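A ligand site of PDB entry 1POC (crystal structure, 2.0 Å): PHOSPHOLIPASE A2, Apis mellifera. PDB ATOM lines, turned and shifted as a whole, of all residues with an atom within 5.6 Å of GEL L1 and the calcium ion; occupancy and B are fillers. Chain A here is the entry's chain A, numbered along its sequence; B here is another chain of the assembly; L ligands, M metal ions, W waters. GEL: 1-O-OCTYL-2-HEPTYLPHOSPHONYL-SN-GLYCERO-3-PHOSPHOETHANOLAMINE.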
ATOM      1  N   ILE A   1     -14.888   4.499 -31.635  1.00  0.00           N
ATOM      2  CA  ILE A   1     -14.402   3.530 -30.622  1.00  0.00           C
ATOM      3  C   ILE A   1     -14.917   3.967 -29.241  1.00  0.00           C
ATOM      4  O   ILE A   1     -14.863   5.151 -28.884  1.00  0.00           O
ATOM      5  CB  ILE A   1     -12.833   3.559 -30.633  1.00  0.00           C
ATOM      6  CG1 ILE A   1     -12.219   2.235 -30.172  1.00  0.00           C
ATOM      7  CG2 ILE A   1     -12.244   4.648 -29.730  1.00  0.00           C
ATOM      8  CD1 ILE A   1     -13.065   1.019 -30.565  1.00  0.00           C
ATOM      9  N   ILE A   2     -15.428   3.000 -28.510  1.00  0.00           N
ATOM     10  CA  ILE A   2     -15.857   3.209 -27.119  1.00  0.00           C
ATOM     11  C   ILE A   2     -15.052   2.237 -26.261  1.00  0.00           C
ATOM     12  O   ILE A   2     -14.907   1.060 -26.603  1.00  0.00           O
ATOM     13  CB  ILE A   2     -17.369   3.021 -26.959  1.00  0.00           C
ATOM     14  CG1 ILE A   2     -18.167   4.249 -27.422  1.00  0.00           C
ATOM     15  CG2 ILE A   2     -17.801   2.800 -25.504  1.00  0.00           C
ATOM     16  CD1 ILE A   2     -19.227   3.911 -28.480  1.00  0.00           C
ATOM     17  N   TYR A   3     -14.541   2.777 -25.180  1.00  0.00           N
ATOM     18  CA  TYR A   3     -13.710   2.017 -24.223  1.00  0.00           C
ATOM     19  C   TYR A   3     -14.586   1.003 -23.487  1.00  0.00           C
ATOM     20  O   TYR A   3     -15.533   1.373 -22.765  1.00  0.00           O
ATOM     21  CB  TYR A   3     -13.070   3.010 -23.250  1.00  0.00           C
ATOM     22  CG  TYR A   3     -12.238   2.361 -22.142  1.00  0.00           C
ATOM     23  CD1 TYR A   3     -11.042   1.689 -22.463  1.00  0.00           C
ATOM     24  CD2 TYR A   3     -12.662   2.434 -20.819  1.00  0.00           C
ATOM     25  CE1 TYR A   3     -10.276   1.121 -21.449  1.00  0.00           C
ATOM     26  CE2 TYR A   3     -11.890   1.859 -19.808  1.00  0.00           C
ATOM     27  CZ  TYR A   3     -10.698   1.204 -20.115  1.00  0.00           C
ATOM     28  OH  TYR A   3      -9.947   0.642 -19.133  1.00  0.00           O
ATOM     29  N   TRP A   8     -20.080   5.667 -22.751  1.00  0.00           N
ATOM     30  CA  TRP A   8     -19.925   7.035 -23.281  1.00  0.00           C
ATOM     31  C   TRP A   8     -18.474   7.467 -23.599  1.00  0.00           C
ATOM     32  O   TRP A   8     -18.240   8.481 -24.273  1.00  0.00           O
ATOM     33  CB  TRP A   8     -20.456   8.050 -22.264  1.00  0.00           C
ATOM     34  CG  TRP A   8     -21.911   7.791 -21.843  1.00  0.00           C
ATOM     35  CD1 TRP A   8     -22.352   6.905 -20.938  1.00  0.00           C
ATOM     36  CD2 TRP A   8     -23.046   8.469 -22.362  1.00  0.00           C
ATOM     37  NE1 TRP A   8     -23.772   7.020 -20.885  1.00  0.00           N
ATOM     38  CE2 TRP A   8     -24.168   7.940 -21.731  1.00  0.00           C
ATOM     39  CE3 TRP A   8     -23.221   9.490 -23.316  1.00  0.00           C
ATOM     40  CZ2 TRP A   8     -25.469   8.370 -21.996  1.00  0.00           C
ATOM     41  CZ3 TRP A   8     -24.533   9.911 -23.581  1.00  0.00           C
ATOM     42  CH2 TRP A   8     -25.613   9.373 -22.950  1.00  0.00           C
ATOM     43  N   CYS A   9     -17.488   6.725 -23.120  1.00  0.00           N
ATOM     44  CA  CYS A   9     -16.064   7.105 -23.354  1.00  0.00           C
ATOM     45  C   CYS A   9     -15.588   6.627 -24.738  1.00  0.00           C
ATOM     46  O   CYS A   9     -15.286   5.439 -24.944  1.00  0.00           O
ATOM     47  CB  CYS A   9     -15.161   6.501 -22.283  1.00  0.00           C
ATOM     48  SG  CYS A   9     -15.591   7.087 -20.578  1.00  0.00           S
ATOM     49  N   GLY A  10     -15.524   7.595 -25.639  1.00  0.00           N
ATOM     50  CA  GLY A  10     -15.106   7.387 -27.050  1.00  0.00           C
ATOM     51  C   GLY A  10     -16.038   8.186 -27.966  1.00  0.00           C
ATOM     52  O   GLY A  10     -16.840   9.004 -27.496  1.00  0.00           O
ATOM     53  N   HIS A  11     -15.917   7.940 -29.265  1.00  0.00           N
ATOM     54  CA  HIS A  11     -16.757   8.614 -30.278  1.00  0.00           C
ATOM     55  C   HIS A  11     -18.223   8.314 -30.022  1.00  0.00           C
ATOM     56  O   HIS A  11     -18.670   7.164 -30.130  1.00  0.00           O
ATOM     57  CB  HIS A  11     -16.463   8.093 -31.684  1.00  0.00           C
ATOM     58  CG  HIS A  11     -15.001   8.240 -32.089  1.00  0.00           C
ATOM     59  ND1 HIS A  11     -14.049   7.294 -31.735  1.00  0.00           N
ATOM     60  CD2 HIS A  11     -14.347   9.184 -32.806  1.00  0.00           C
ATOM     61  CE1 HIS A  11     -12.888   7.677 -32.216  1.00  0.00           C
ATOM     62  NE2 HIS A  11     -13.045   8.806 -32.864  1.00  0.00           N
ATOM     63  N   GLY A  12     -18.948   9.361 -29.692  1.00  0.00           N
ATOM     64  CA  GLY A  12     -20.378   9.270 -29.395  1.00  0.00           C
ATOM     65  C   GLY A  12     -20.574   8.444 -28.132  1.00  0.00           C
ATOM     66  O   GLY A  12     -19.823   8.589 -27.147  1.00  0.00           O
ATOM     67  N   ASN A  13     -21.581   7.604 -28.181  1.00  0.00           N
ATOM     68  CA  ASN A  13     -21.943   6.719 -27.067  1.00  0.00           C
ATOM     69  C   ASN A  13     -22.717   5.518 -27.614  1.00  0.00           C
ATOM     70  O   ASN A  13     -23.254   5.565 -28.731  1.00  0.00           O
ATOM     71  CB  ASN A  13     -22.833   7.493 -26.078  1.00  0.00           C
ATOM     72  CG  ASN A  13     -24.264   7.697 -26.586  1.00  0.00           C
ATOM     73  OD1 ASN A  13     -25.130   6.865 -26.326  1.00  0.00           O
ATOM     74  ND2 ASN A  13     -24.581   8.764 -27.292  1.00  0.00           N
ATOM     75  N   CYS A  30     -18.267  10.577 -15.917  1.00  0.00           N
ATOM     76  CA  CYS A  30     -17.429  11.719 -16.285  1.00  0.00           C
ATOM     77  C   CYS A  30     -17.528  11.940 -17.825  1.00  0.00           C
ATOM     78  O   CYS A  30     -17.564  13.083 -18.304  1.00  0.00           O
ATOM     79  CB  CYS A  30     -15.997  11.467 -15.762  1.00  0.00           C
ATOM     80  SG  CYS A  30     -15.835  11.893 -13.970  1.00  0.00           S
ATOM     81  N   CYS A  31     -17.593  10.841 -18.583  1.00  0.00           N
ATOM     82  CA  CYS A  31     -17.678  10.908 -20.069  1.00  0.00           C
ATOM     83  C   CYS A  31     -19.089  11.298 -20.539  1.00  0.00           C
ATOM     84  O   CYS A  31     -19.264  12.004 -21.540  1.00  0.00           O
ATOM     85  CB  CYS A  31     -17.335   9.555 -20.694  1.00  0.00           C
ATOM     86  SG  CYS A  31     -15.557   9.096 -20.444  1.00  0.00           S
ATOM     87  N   HIS A  34     -19.447  14.878 -20.150  1.00  0.00           N
ATOM     88  CA  HIS A  34     -18.552  15.450 -21.179  1.00  0.00           C
ATOM     89  C   HIS A  34     -19.288  15.511 -22.526  1.00  0.00           C
ATOM     90  O   HIS A  34     -19.286  16.536 -23.215  1.00  0.00           O
ATOM     91  CB  HIS A  34     -17.283  14.589 -21.297  1.00  0.00           C
ATOM     92  CG  HIS A  34     -16.120  15.303 -22.011  1.00  0.00           C
ATOM     93  ND1 HIS A  34     -15.307  14.645 -22.918  1.00  0.00           N
ATOM     94  CD2 HIS A  34     -15.655  16.579 -21.936  1.00  0.00           C
ATOM     95  CE1 HIS A  34     -14.407  15.494 -23.367  1.00  0.00           C
ATOM     96  NE2 HIS A  34     -14.593  16.654 -22.795  1.00  0.00           N
ATOM     97  N   ASP A  35     -19.922  14.394 -22.856  1.00  0.00           N
ATOM     98  CA  ASP A  35     -20.672  14.246 -24.112  1.00  0.00           C
ATOM     99  C   ASP A  35     -21.884  15.197 -24.159  1.00  0.00           C
ATOM    100  O   ASP A  35     -22.343  15.596 -25.238  1.00  0.00           O
ATOM    101  CB  ASP A  35     -21.202  12.808 -24.258  1.00  0.00           C
ATOM    102  CG  ASP A  35     -20.193  11.832 -24.854  1.00  0.00           C
ATOM    103  OD1 ASP A  35     -18.929  12.052 -24.762  1.00  0.00           O
ATOM    104  OD2 ASP A  35     -20.610  10.767 -25.460  1.00  0.00           O
ATOM    105  N   MET A  36     -22.389  15.530 -22.975  1.00  0.00           N
ATOM    106  CA  MET A  36     -23.603  16.366 -22.835  1.00  0.00           C
ATOM    107  C   MET A  36     -23.262  17.862 -22.708  1.00  0.00           C
ATOM    108  O   MET A  36     -24.118  18.676 -22.331  1.00  0.00           O
ATOM    109  CB  MET A  36     -24.392  15.911 -21.622  1.00  0.00           C
ATOM    110  CG  MET A  36     -25.238  14.676 -21.928  1.00  0.00           C
ATOM    111  SD  MET A  36     -26.066  13.992 -20.523  1.00  0.00           S
ATOM    112  CE  MET A  36     -26.818  12.454 -20.992  1.00  0.00           C
ATOM    113  N   VAL A  40     -20.396  22.204 -28.324  1.00  0.00           N
ATOM    114  CA  VAL A  40     -19.446  21.311 -29.007  1.00  0.00           C
ATOM    115  C   VAL A  40     -19.543  21.532 -30.517  1.00  0.00           C
ATOM    116  O   VAL A  40     -20.549  22.054 -31.022  1.00  0.00           O
ATOM    117  CB  VAL A  40     -19.834  19.836 -28.782  1.00  0.00           C
ATOM    118  CG1 VAL A  40     -19.820  19.431 -27.299  1.00  0.00           C
ATOM    119  CG2 VAL A  40     -21.239  19.499 -29.286  1.00  0.00           C
ATOM    120  N   HIS A  56     -12.585  13.958 -34.840  1.00  0.00           N
ATOM    121  CA  HIS A  56     -13.386  13.773 -33.614  1.00  0.00           C
ATOM    122  C   HIS A  56     -13.935  15.121 -33.139  1.00  0.00           C
ATOM    123  O   HIS A  56     -13.490  16.187 -33.588  1.00  0.00           O
ATOM    124  CB  HIS A  56     -12.609  13.036 -32.472  1.00  0.00           C
ATOM    125  CG  HIS A  56     -11.229  13.576 -32.027  1.00  0.00           C
ATOM    126  ND1 HIS A  56     -11.091  14.581 -31.067  1.00  0.00           N
ATOM    127  CD2 HIS A  56      -9.952  13.238 -32.372  1.00  0.00           C
ATOM    128  CE1 HIS A  56      -9.803  14.799 -30.860  1.00  0.00           C
ATOM    129  NE2 HIS A  56      -9.113  14.006 -31.636  1.00  0.00           N
ATOM    130  N   THR A  57     -14.895  15.008 -32.245  1.00  0.00           N
ATOM    131  CA  THR A  57     -15.569  16.163 -31.665  1.00  0.00           C
ATOM    132  C   THR A  57     -14.602  16.948 -30.783  1.00  0.00           C
ATOM    133  O   THR A  57     -13.760  16.368 -30.095  1.00  0.00           O
ATOM    134  CB  THR A  57     -16.730  15.710 -30.775  1.00  0.00           C
ATOM    135  OG1 THR A  57     -17.681  14.981 -31.536  1.00  0.00           O
ATOM    136  CG2 THR A  57     -17.471  16.876 -30.103  1.00  0.00           C
ATOM    137  N   LEU A  59     -14.783  20.236 -28.029  1.00  0.00           N
ATOM    138  CA  LEU A  59     -15.712  21.029 -27.207  1.00  0.00           C
ATOM    139  C   LEU A  59     -15.051  22.253 -26.582  1.00  0.00           C
ATOM    140  O   LEU A  59     -13.830  22.440 -26.666  1.00  0.00           O
ATOM    141  CB  LEU A  59     -16.284  20.233 -26.020  1.00  0.00           C
ATOM    142  CG  LEU A  59     -15.863  18.758 -25.929  1.00  0.00           C
ATOM    143  CD1 LEU A  59     -16.970  17.884 -25.320  1.00  0.00           C
ATOM    144  CD2 LEU A  59     -15.543  18.114 -27.274  1.00  0.00           C
ATOM    145  N   PHE A  67     -14.177  17.941 -17.229  1.00  0.00           N
ATOM    146  CA  PHE A  67     -13.915  16.533 -17.563  1.00  0.00           C
ATOM    147  C   PHE A  67     -12.615  16.079 -16.874  1.00  0.00           C
ATOM    148  O   PHE A  67     -12.525  14.974 -16.314  1.00  0.00           O
ATOM    149  CB  PHE A  67     -13.787  16.382 -19.080  1.00  0.00           C
ATOM    150  CG  PHE A  67     -13.673  14.926 -19.557  1.00  0.00           C
ATOM    151  CD1 PHE A  67     -14.496  13.937 -19.021  1.00  0.00           C
ATOM    152  CD2 PHE A  67     -12.734  14.587 -20.551  1.00  0.00           C
ATOM    153  CE1 PHE A  67     -14.387  12.606 -19.456  1.00  0.00           C
ATOM    154  CE2 PHE A  67     -12.621  13.262 -20.993  1.00  0.00           C
ATOM    155  CZ  PHE A  67     -13.446  12.276 -20.441  1.00  0.00           C
ATOM    156  N   PHE A  82      -6.454   5.801 -17.607  1.00  0.00           N
ATOM    157  CA  PHE A  82      -6.275   5.416 -19.022  1.00  0.00           C
ATOM    158  C   PHE A  82      -6.990   6.409 -19.945  1.00  0.00           C
ATOM    159  O   PHE A  82      -6.427   6.878 -20.943  1.00  0.00           O
ATOM    160  CB  PHE A  82      -6.813   4.016 -19.300  1.00  0.00           C
ATOM    161  CG  PHE A  82      -6.701   3.645 -20.784  1.00  0.00           C
ATOM    162  CD1 PHE A  82      -5.473   3.199 -21.303  1.00  0.00           C
ATOM    163  CD2 PHE A  82      -7.816   3.759 -21.620  1.00  0.00           C
ATOM    164  CE1 PHE A  82      -5.370   2.880 -22.667  1.00  0.00           C
ATOM    165  CE2 PHE A  82      -7.706   3.455 -22.980  1.00  0.00           C
ATOM    166  CZ  PHE A  82      -6.475   3.016 -23.506  1.00  0.00           C
ATOM    167  N   VAL A  83      -8.224   6.715 -19.607  1.00  0.00           N
ATOM    168  CA  VAL A  83      -9.051   7.638 -20.405  1.00  0.00           C
ATOM    169  C   VAL A  83      -8.493   9.060 -20.318  1.00  0.00           C
ATOM    170  O   VAL A  83      -8.528   9.818 -21.297  1.00  0.00           O
ATOM    171  CB  VAL A  83     -10.506   7.589 -19.918  1.00  0.00           C
ATOM    172  CG1 VAL A  83     -11.370   8.698 -20.530  1.00  0.00           C
ATOM    173  CG2 VAL A  83     -11.205   6.279 -20.259  1.00  0.00           C
ATOM    174  N   MET A  86      -5.065   9.290 -22.309  1.00  0.00           N
ATOM    175  CA  MET A  86      -5.377   9.191 -23.753  1.00  0.00           C
ATOM    176  C   MET A  86      -5.902  10.523 -24.306  1.00  0.00           C
ATOM    177  O   MET A  86      -5.359  11.065 -25.290  1.00  0.00           O
ATOM    178  CB  MET A  86      -6.452   8.139 -24.011  1.00  0.00           C
ATOM    179  CG  MET A  86      -5.909   6.710 -23.987  1.00  0.00           C
ATOM    180  SD  MET A  86      -5.151   6.229 -25.529  1.00  0.00           S
ATOM    181  CE  MET A  86      -5.883   7.153 -26.855  1.00  0.00           C
ATOM    182  N   TYR A  87      -6.939  11.018 -23.664  1.00  0.00           N
ATOM    183  CA  TYR A  87      -7.643  12.240 -24.110  1.00  0.00           C
ATOM    184  C   TYR A  87      -6.807  13.524 -23.985  1.00  0.00           C
ATOM    185  O   TYR A  87      -6.739  14.325 -24.926  1.00  0.00           O
ATOM    186  CB  TYR A  87      -8.920  12.465 -23.277  1.00  0.00           C
ATOM    187  CG  TYR A  87      -9.782  13.609 -23.825  1.00  0.00           C
ATOM    188  CD1 TYR A  87     -10.599  13.393 -24.945  1.00  0.00           C
ATOM    189  CD2 TYR A  87      -9.751  14.871 -23.214  1.00  0.00           C
ATOM    190  CE1 TYR A  87     -11.370  14.433 -25.452  1.00  0.00           C
ATOM    191  CE2 TYR A  87     -10.529  15.909 -23.727  1.00  0.00           C
ATOM    192  CZ  TYR A  87     -11.346  15.692 -24.847  1.00  0.00           C
ATOM    193  OH  TYR A  87     -12.102  16.714 -25.349  1.00  0.00           O
ATOM    194  N   ILE A  91      -4.023  12.157 -27.811  1.00  0.00           N
ATOM    195  CA  ILE A  91      -4.760  12.408 -29.082  1.00  0.00           C
ATOM    196  C   ILE A  91      -4.551  13.820 -29.644  1.00  0.00           C
ATOM    197  O   ILE A  91      -4.988  14.143 -30.754  1.00  0.00           O
ATOM    198  CB  ILE A  91      -6.267  12.156 -28.921  1.00  0.00           C
ATOM    199  CG1 ILE A  91      -6.918  13.041 -27.857  1.00  0.00           C
ATOM    200  CG2 ILE A  91      -6.580  10.707 -28.541  1.00  0.00           C
ATOM    201  CD1 ILE A  91      -8.445  13.022 -27.932  1.00  0.00           C
ATOM    202  N   PHE B  82     -11.243  -3.833 -29.449  1.00  0.00           N
ATOM    203  CA  PHE B  82     -10.849  -2.461 -29.069  1.00  0.00           C
ATOM    204  C   PHE B  82      -9.397  -2.185 -29.476  1.00  0.00           C
ATOM    205  O   PHE B  82      -9.082  -1.143 -30.064  1.00  0.00           O
ATOM    206  CB  PHE B  82     -10.988  -2.228 -27.568  1.00  0.00           C
ATOM    207  CG  PHE B  82     -10.505  -0.831 -27.160  1.00  0.00           C
ATOM    208  CD1 PHE B  82     -11.345   0.281 -27.339  1.00  0.00           C
ATOM    209  CD2 PHE B  82      -9.227  -0.663 -26.619  1.00  0.00           C
ATOM    210  CE1 PHE B  82     -10.891   1.561 -26.982  1.00  0.00           C
ATOM    211  CE2 PHE B  82      -8.770   0.614 -26.280  1.00  0.00           C
ATOM    212  CZ  PHE B  82      -9.607   1.732 -26.466  1.00  0.00           C
ATOM    213  N   MET B  86      -8.235   0.251 -32.687  1.00  0.00           N
ATOM    214  CA  MET B  86      -7.335   1.362 -32.305  1.00  0.00           C
ATOM    215  C   MET B  86      -6.044   1.350 -33.135  1.00  0.00           C
ATOM    216  O   MET B  86      -5.687   2.358 -33.777  1.00  0.00           O
ATOM    217  CB  MET B  86      -6.929   1.260 -30.837  1.00  0.00           C
ATOM    218  CG  MET B  86      -8.016   1.754 -29.881  1.00  0.00           C
ATOM    219  SD  MET B  86      -8.022   3.529 -29.695  1.00  0.00           S
ATOM    220  CE  MET B  86      -6.390   4.155 -29.995  1.00  0.00           C
ATOM    221  N   LEU B  90      -7.292   3.605 -36.141  1.00  0.00           N
ATOM    222  CA  LEU B  90      -7.321   4.967 -35.573  1.00  0.00           C
ATOM    223  C   LEU B  90      -5.967   5.678 -35.380  1.00  0.00           C
ATOM    224  O   LEU B  90      -5.870   6.914 -35.443  1.00  0.00           O
ATOM    225  CB  LEU B  90      -8.039   4.936 -34.213  1.00  0.00           C
ATOM    226  CG  LEU B  90      -9.502   4.510 -34.329  1.00  0.00           C
ATOM    227  CD1 LEU B  90     -10.178   4.332 -32.967  1.00  0.00           C
ATOM    228  CD2 LEU B  90     -10.362   5.524 -35.088  1.00  0.00           C
ATOM    229  N   ILE B  91      -4.872   4.969 -35.138  1.00  0.00           N
ATOM    230  CA  ILE B  91      -3.584   5.666 -34.861  1.00  0.00           C
ATOM    231  C   ILE B  91      -2.781   5.997 -36.126  1.00  0.00           C
ATOM    232  O   ILE B  91      -1.757   6.686 -36.077  1.00  0.00           O
ATOM    233  CB  ILE B  91      -2.695   4.855 -33.907  1.00  0.00           C
ATOM    234  CG1 ILE B  91      -2.339   3.477 -34.443  1.00  0.00           C
ATOM    235  CG2 ILE B  91      -3.349   4.638 -32.541  1.00  0.00           C
ATOM    236  CD1 ILE B  91      -1.201   2.810 -33.660  1.00  0.00           C
HETATM  237  C1  GEL L   1     -14.557  13.444 -27.669  1.00  0.00           C
HETATM  238  O1  GEL L   1     -13.365  12.609 -27.641  1.00  0.00           O
HETATM  239  C11 GEL L   1     -13.334  11.924 -28.932  1.00  0.00           C
HETATM  240  C12 GEL L   1     -12.557  10.614 -28.829  1.00  0.00           C
HETATM  241  C13 GEL L   1     -11.509  10.383 -29.897  1.00  0.00           C
HETATM  242  C14 GEL L   1     -10.864   9.016 -29.921  1.00  0.00           C
HETATM  243  C15 GEL L   1      -9.416   8.999 -30.297  1.00  0.00           C
HETATM  244  C16 GEL L   1      -8.849   7.813 -30.994  1.00  0.00           C
HETATM  245  C17 GEL L   1      -7.517   8.010 -31.676  1.00  0.00           C
HETATM  246  C18 GEL L   1      -6.464   6.945 -31.336  1.00  0.00           C
HETATM  247  C2  GEL L   1     -15.591  12.886 -26.734  1.00  0.00           C
HETATM  248  O2  GEL L   1     -14.989  12.575 -25.490  1.00  0.00           O
HETATM  249  P2  GEL L   1     -15.306  11.362 -24.487  1.00  0.00           P
HETATM  250  O1P GEL L   1     -15.696  12.013 -23.203  1.00  0.00           O
HETATM  251  O2P GEL L   1     -16.328  10.479 -25.061  1.00  0.00           O
HETATM  252  C22 GEL L   1     -13.573  10.969 -24.750  1.00  0.00           C
HETATM  253  C23 GEL L   1     -12.922   9.712 -24.516  1.00  0.00           C
HETATM  254  C24 GEL L   1     -11.600   9.324 -25.137  1.00  0.00           C
HETATM  255  C25 GEL L   1     -11.070   8.096 -24.466  1.00  0.00           C
HETATM  256  C26 GEL L   1     -10.251   7.074 -25.092  1.00  0.00           C
HETATM  257  C27 GEL L   1     -10.714   5.632 -24.982  1.00  0.00           C
HETATM  258  C28 GEL L   1     -10.907   5.035 -26.372  1.00  0.00           C
HETATM  259  C3  GEL L   1     -16.799  13.784 -26.576  1.00  0.00           C
HETATM  260  O3  GEL L   1     -17.408  13.915 -27.875  1.00  0.00           O
HETATM  261  P3  GEL L   1     -18.594  12.890 -28.363  1.00  0.00           P
HETATM  262  O3P GEL L   1     -18.499  12.864 -29.854  1.00  0.00           O
HETATM  263  O4P GEL L   1     -18.488  11.596 -27.707  1.00  0.00           O
HETATM  264  O5P GEL L   1     -19.616  13.915 -27.848  1.00  0.00           O
HETATM  265  C31 GEL L   1     -21.001  13.807 -27.661  1.00  0.00           C
HETATM  266  C32 GEL L   1     -21.688  14.907 -28.466  1.00  0.00           C
HETATM  267  N3  GEL L   1     -22.802  14.205 -29.201  1.00  0.00           N
HETATM  268  C1  GEL L   2       3.289  -0.405 -30.994  1.00  0.00           C
HETATM  269  O1  GEL L   2       2.015   0.288 -30.875  1.00  0.00           O
HETATM  270  C11 GEL L   2       2.311   1.537 -30.175  1.00  0.00           C
HETATM  271  C12 GEL L   2       1.073   2.053 -29.445  1.00  0.00           C
HETATM  272  C13 GEL L   2       0.739   3.514 -29.666  1.00  0.00           C
HETATM  273  C14 GEL L   2      -0.368   4.087 -28.810  1.00  0.00           C
HETATM  274  C15 GEL L   2      -1.235   5.103 -29.482  1.00  0.00           C
HETATM  275  C16 GEL L   2      -1.862   6.187 -28.677  1.00  0.00           C
HETATM  276  C17 GEL L   2      -2.390   7.373 -29.445  1.00  0.00           C
HETATM  277  C18 GEL L   2      -3.830   7.773 -29.087  1.00  0.00           C
HETATM  278  C2  GEL L   2       3.303  -1.602 -30.089  1.00  0.00           C
HETATM  279  O2  GEL L   2       2.098  -2.330 -30.244  1.00  0.00           O
HETATM  280  P2  GEL L   2       1.248  -3.128 -29.139  1.00  0.00           P
HETATM  281  O1P GEL L   2       1.199  -4.535 -29.630  1.00  0.00           O
HETATM  282  O2P GEL L   2       1.853  -2.963 -27.813  1.00  0.00           O
HETATM  283  C22 GEL L   2      -0.062  -2.005 -29.642  1.00  0.00           C
HETATM  284  C23 GEL L   2      -1.248  -1.671 -28.908  1.00  0.00           C
HETATM  285  C24 GEL L   2      -2.079  -0.437 -29.174  1.00  0.00           C
HETATM  286  C25 GEL L   2      -3.383  -0.541 -28.447  1.00  0.00           C
HETATM  287  C26 GEL L   2      -4.150   0.570 -27.916  1.00  0.00           C
HETATM  288  C27 GEL L   2      -4.558   0.513 -26.454  1.00  0.00           C
HETATM  289  C28 GEL L   2      -4.008   1.725 -25.709  1.00  0.00           C
HETATM  290  C3  GEL L   2       4.526  -2.476 -30.274  1.00  0.00           C
HETATM  291  O3  GEL L   2       5.679  -1.671 -29.955  1.00  0.00           O
HETATM  292  P3  GEL L   2       6.291  -1.633 -28.433  1.00  0.00           P
HETATM  293  O3P GEL L   2       6.955  -0.299 -28.312  1.00  0.00           O
HETATM  294  O4P GEL L   2       5.270  -1.915 -27.437  1.00  0.00           O
HETATM  295  O5P GEL L   2       7.261  -2.747 -28.854  1.00  0.00           O
HETATM  296  C31 GEL L   2       8.118  -3.549 -28.087  1.00  0.00           C
HETATM  297  C32 GEL L   2       9.542  -3.381 -28.613  1.00  0.00           C
HETATM  298  N3  GEL L   2      10.381  -3.153 -27.380  1.00  0.00           N
HETATM  299 CA    CA M   1     -18.381  10.055 -26.007  1.00  0.00          CA
HETATM  300  O   HOH W   1     -22.367  10.783 -27.267  1.00  0.00           O
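Of the 28 residues printed, 4 come within 4 Å of the calcium ion.
O4P of GEL L1 binds the calcium ion (2.3 Å). An oxygen (O2P) of GEL L1 binds the calcium ion, at 2.3 Å. The calcium ion is bound by the backbone carbonyl oxygen (O) of Trp 8. The calcium ion is bound by O of Gly 12, 2.4 Å away. The calcium ion is bound by the backbone carbonyl oxygen (O) of Gly 10, 2.4 Å away. The calcium ion is bound by the side-chain carboxylate (OD2) of Asp 35, 2.4 Å away. The calcium ion is bound by OD1 of Asp 35 (2.4 Å).
The backbone carbonyl oxygen (O) of Met 86 of chain B sits at hydrogen-bond distance from the backbone NH (N) of Ile 91 of chain B. The backbone NH of Ile 1 is in hydrogen-bond range of a ring nitrogen (ND1) of His 11, at 2.9 Å. The backbone carbonyl oxygen of Met 86 of chain A is in hydrogen-bond range of the backbone NH of Ile 91 of chain A (3.1 Å). The side-chain sulfur of Cys 9 forms a disulfide with the side-chain sulfur of Cys 31, 2.0 Å away. The backbone carbonyl oxygen (O) of Cys 9 is in hydrogen-bond range of the backbone NH (N) of Tyr 3.
N of Gly 12 lies close to O4P of GEL L1, at 3.0 Å. An oxygen (O2P) of GEL L1 sits close to the backbone NH of Gly 10 (3.0 Å). O1P of GEL L1 is in hydrogen-bond range of ND1 of His 34 (2.7 Å). An oxygen (O3P) of GEL L1 lies within hydrogen-bond range of the side-chain hydroxyl of Thr 57 (2.8 Å).
Residues that only touch GEL L1: Met 86 of chain B (3.1 Å), His 11 (3.3 Å), Tyr 87 (3.5 Å), Phe 82 of chain B (3.5 Å), Phe 67 (3.6 Å), Ile 1 (3.6 Å), Ile 91 of chain A (3.7 Å), His 56 (3.8 Å), Cys 9 (3.8 Å), Leu 90 of chain B (3.8 Å), Cys 31 (3.9 Å), Tyr 3 (3.9 Å) and Val 83 (3.99 Å). Hydrophobic or aromatic side chains within 4 Å of GEL L1: Ile 1, Tyr 3, His 11, His 34, His 56, Phe 67, Val 83, Tyr 87, Ile 91 of chain A, Phe 82 of chain B, Met 86 of chain B and Leu 90 of chain B. 19 residues have an atom within 4 Å of GEL L1: Ile 1, Tyr 3, Trp 8, Cys 9, Gly 10, His 11, Gly 12, Cys 31, His 34, Asp 35, His 56, Thr 57, Phe 67, Val 83, Tyr 87, Ile 91 of chain A, Phe 82 of chain B, Met 86 of chain B and Leu 90 of chain B. The nearest printed residue that does not touch GEL L1 is Ile 91 of chain B (4.1 Å).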
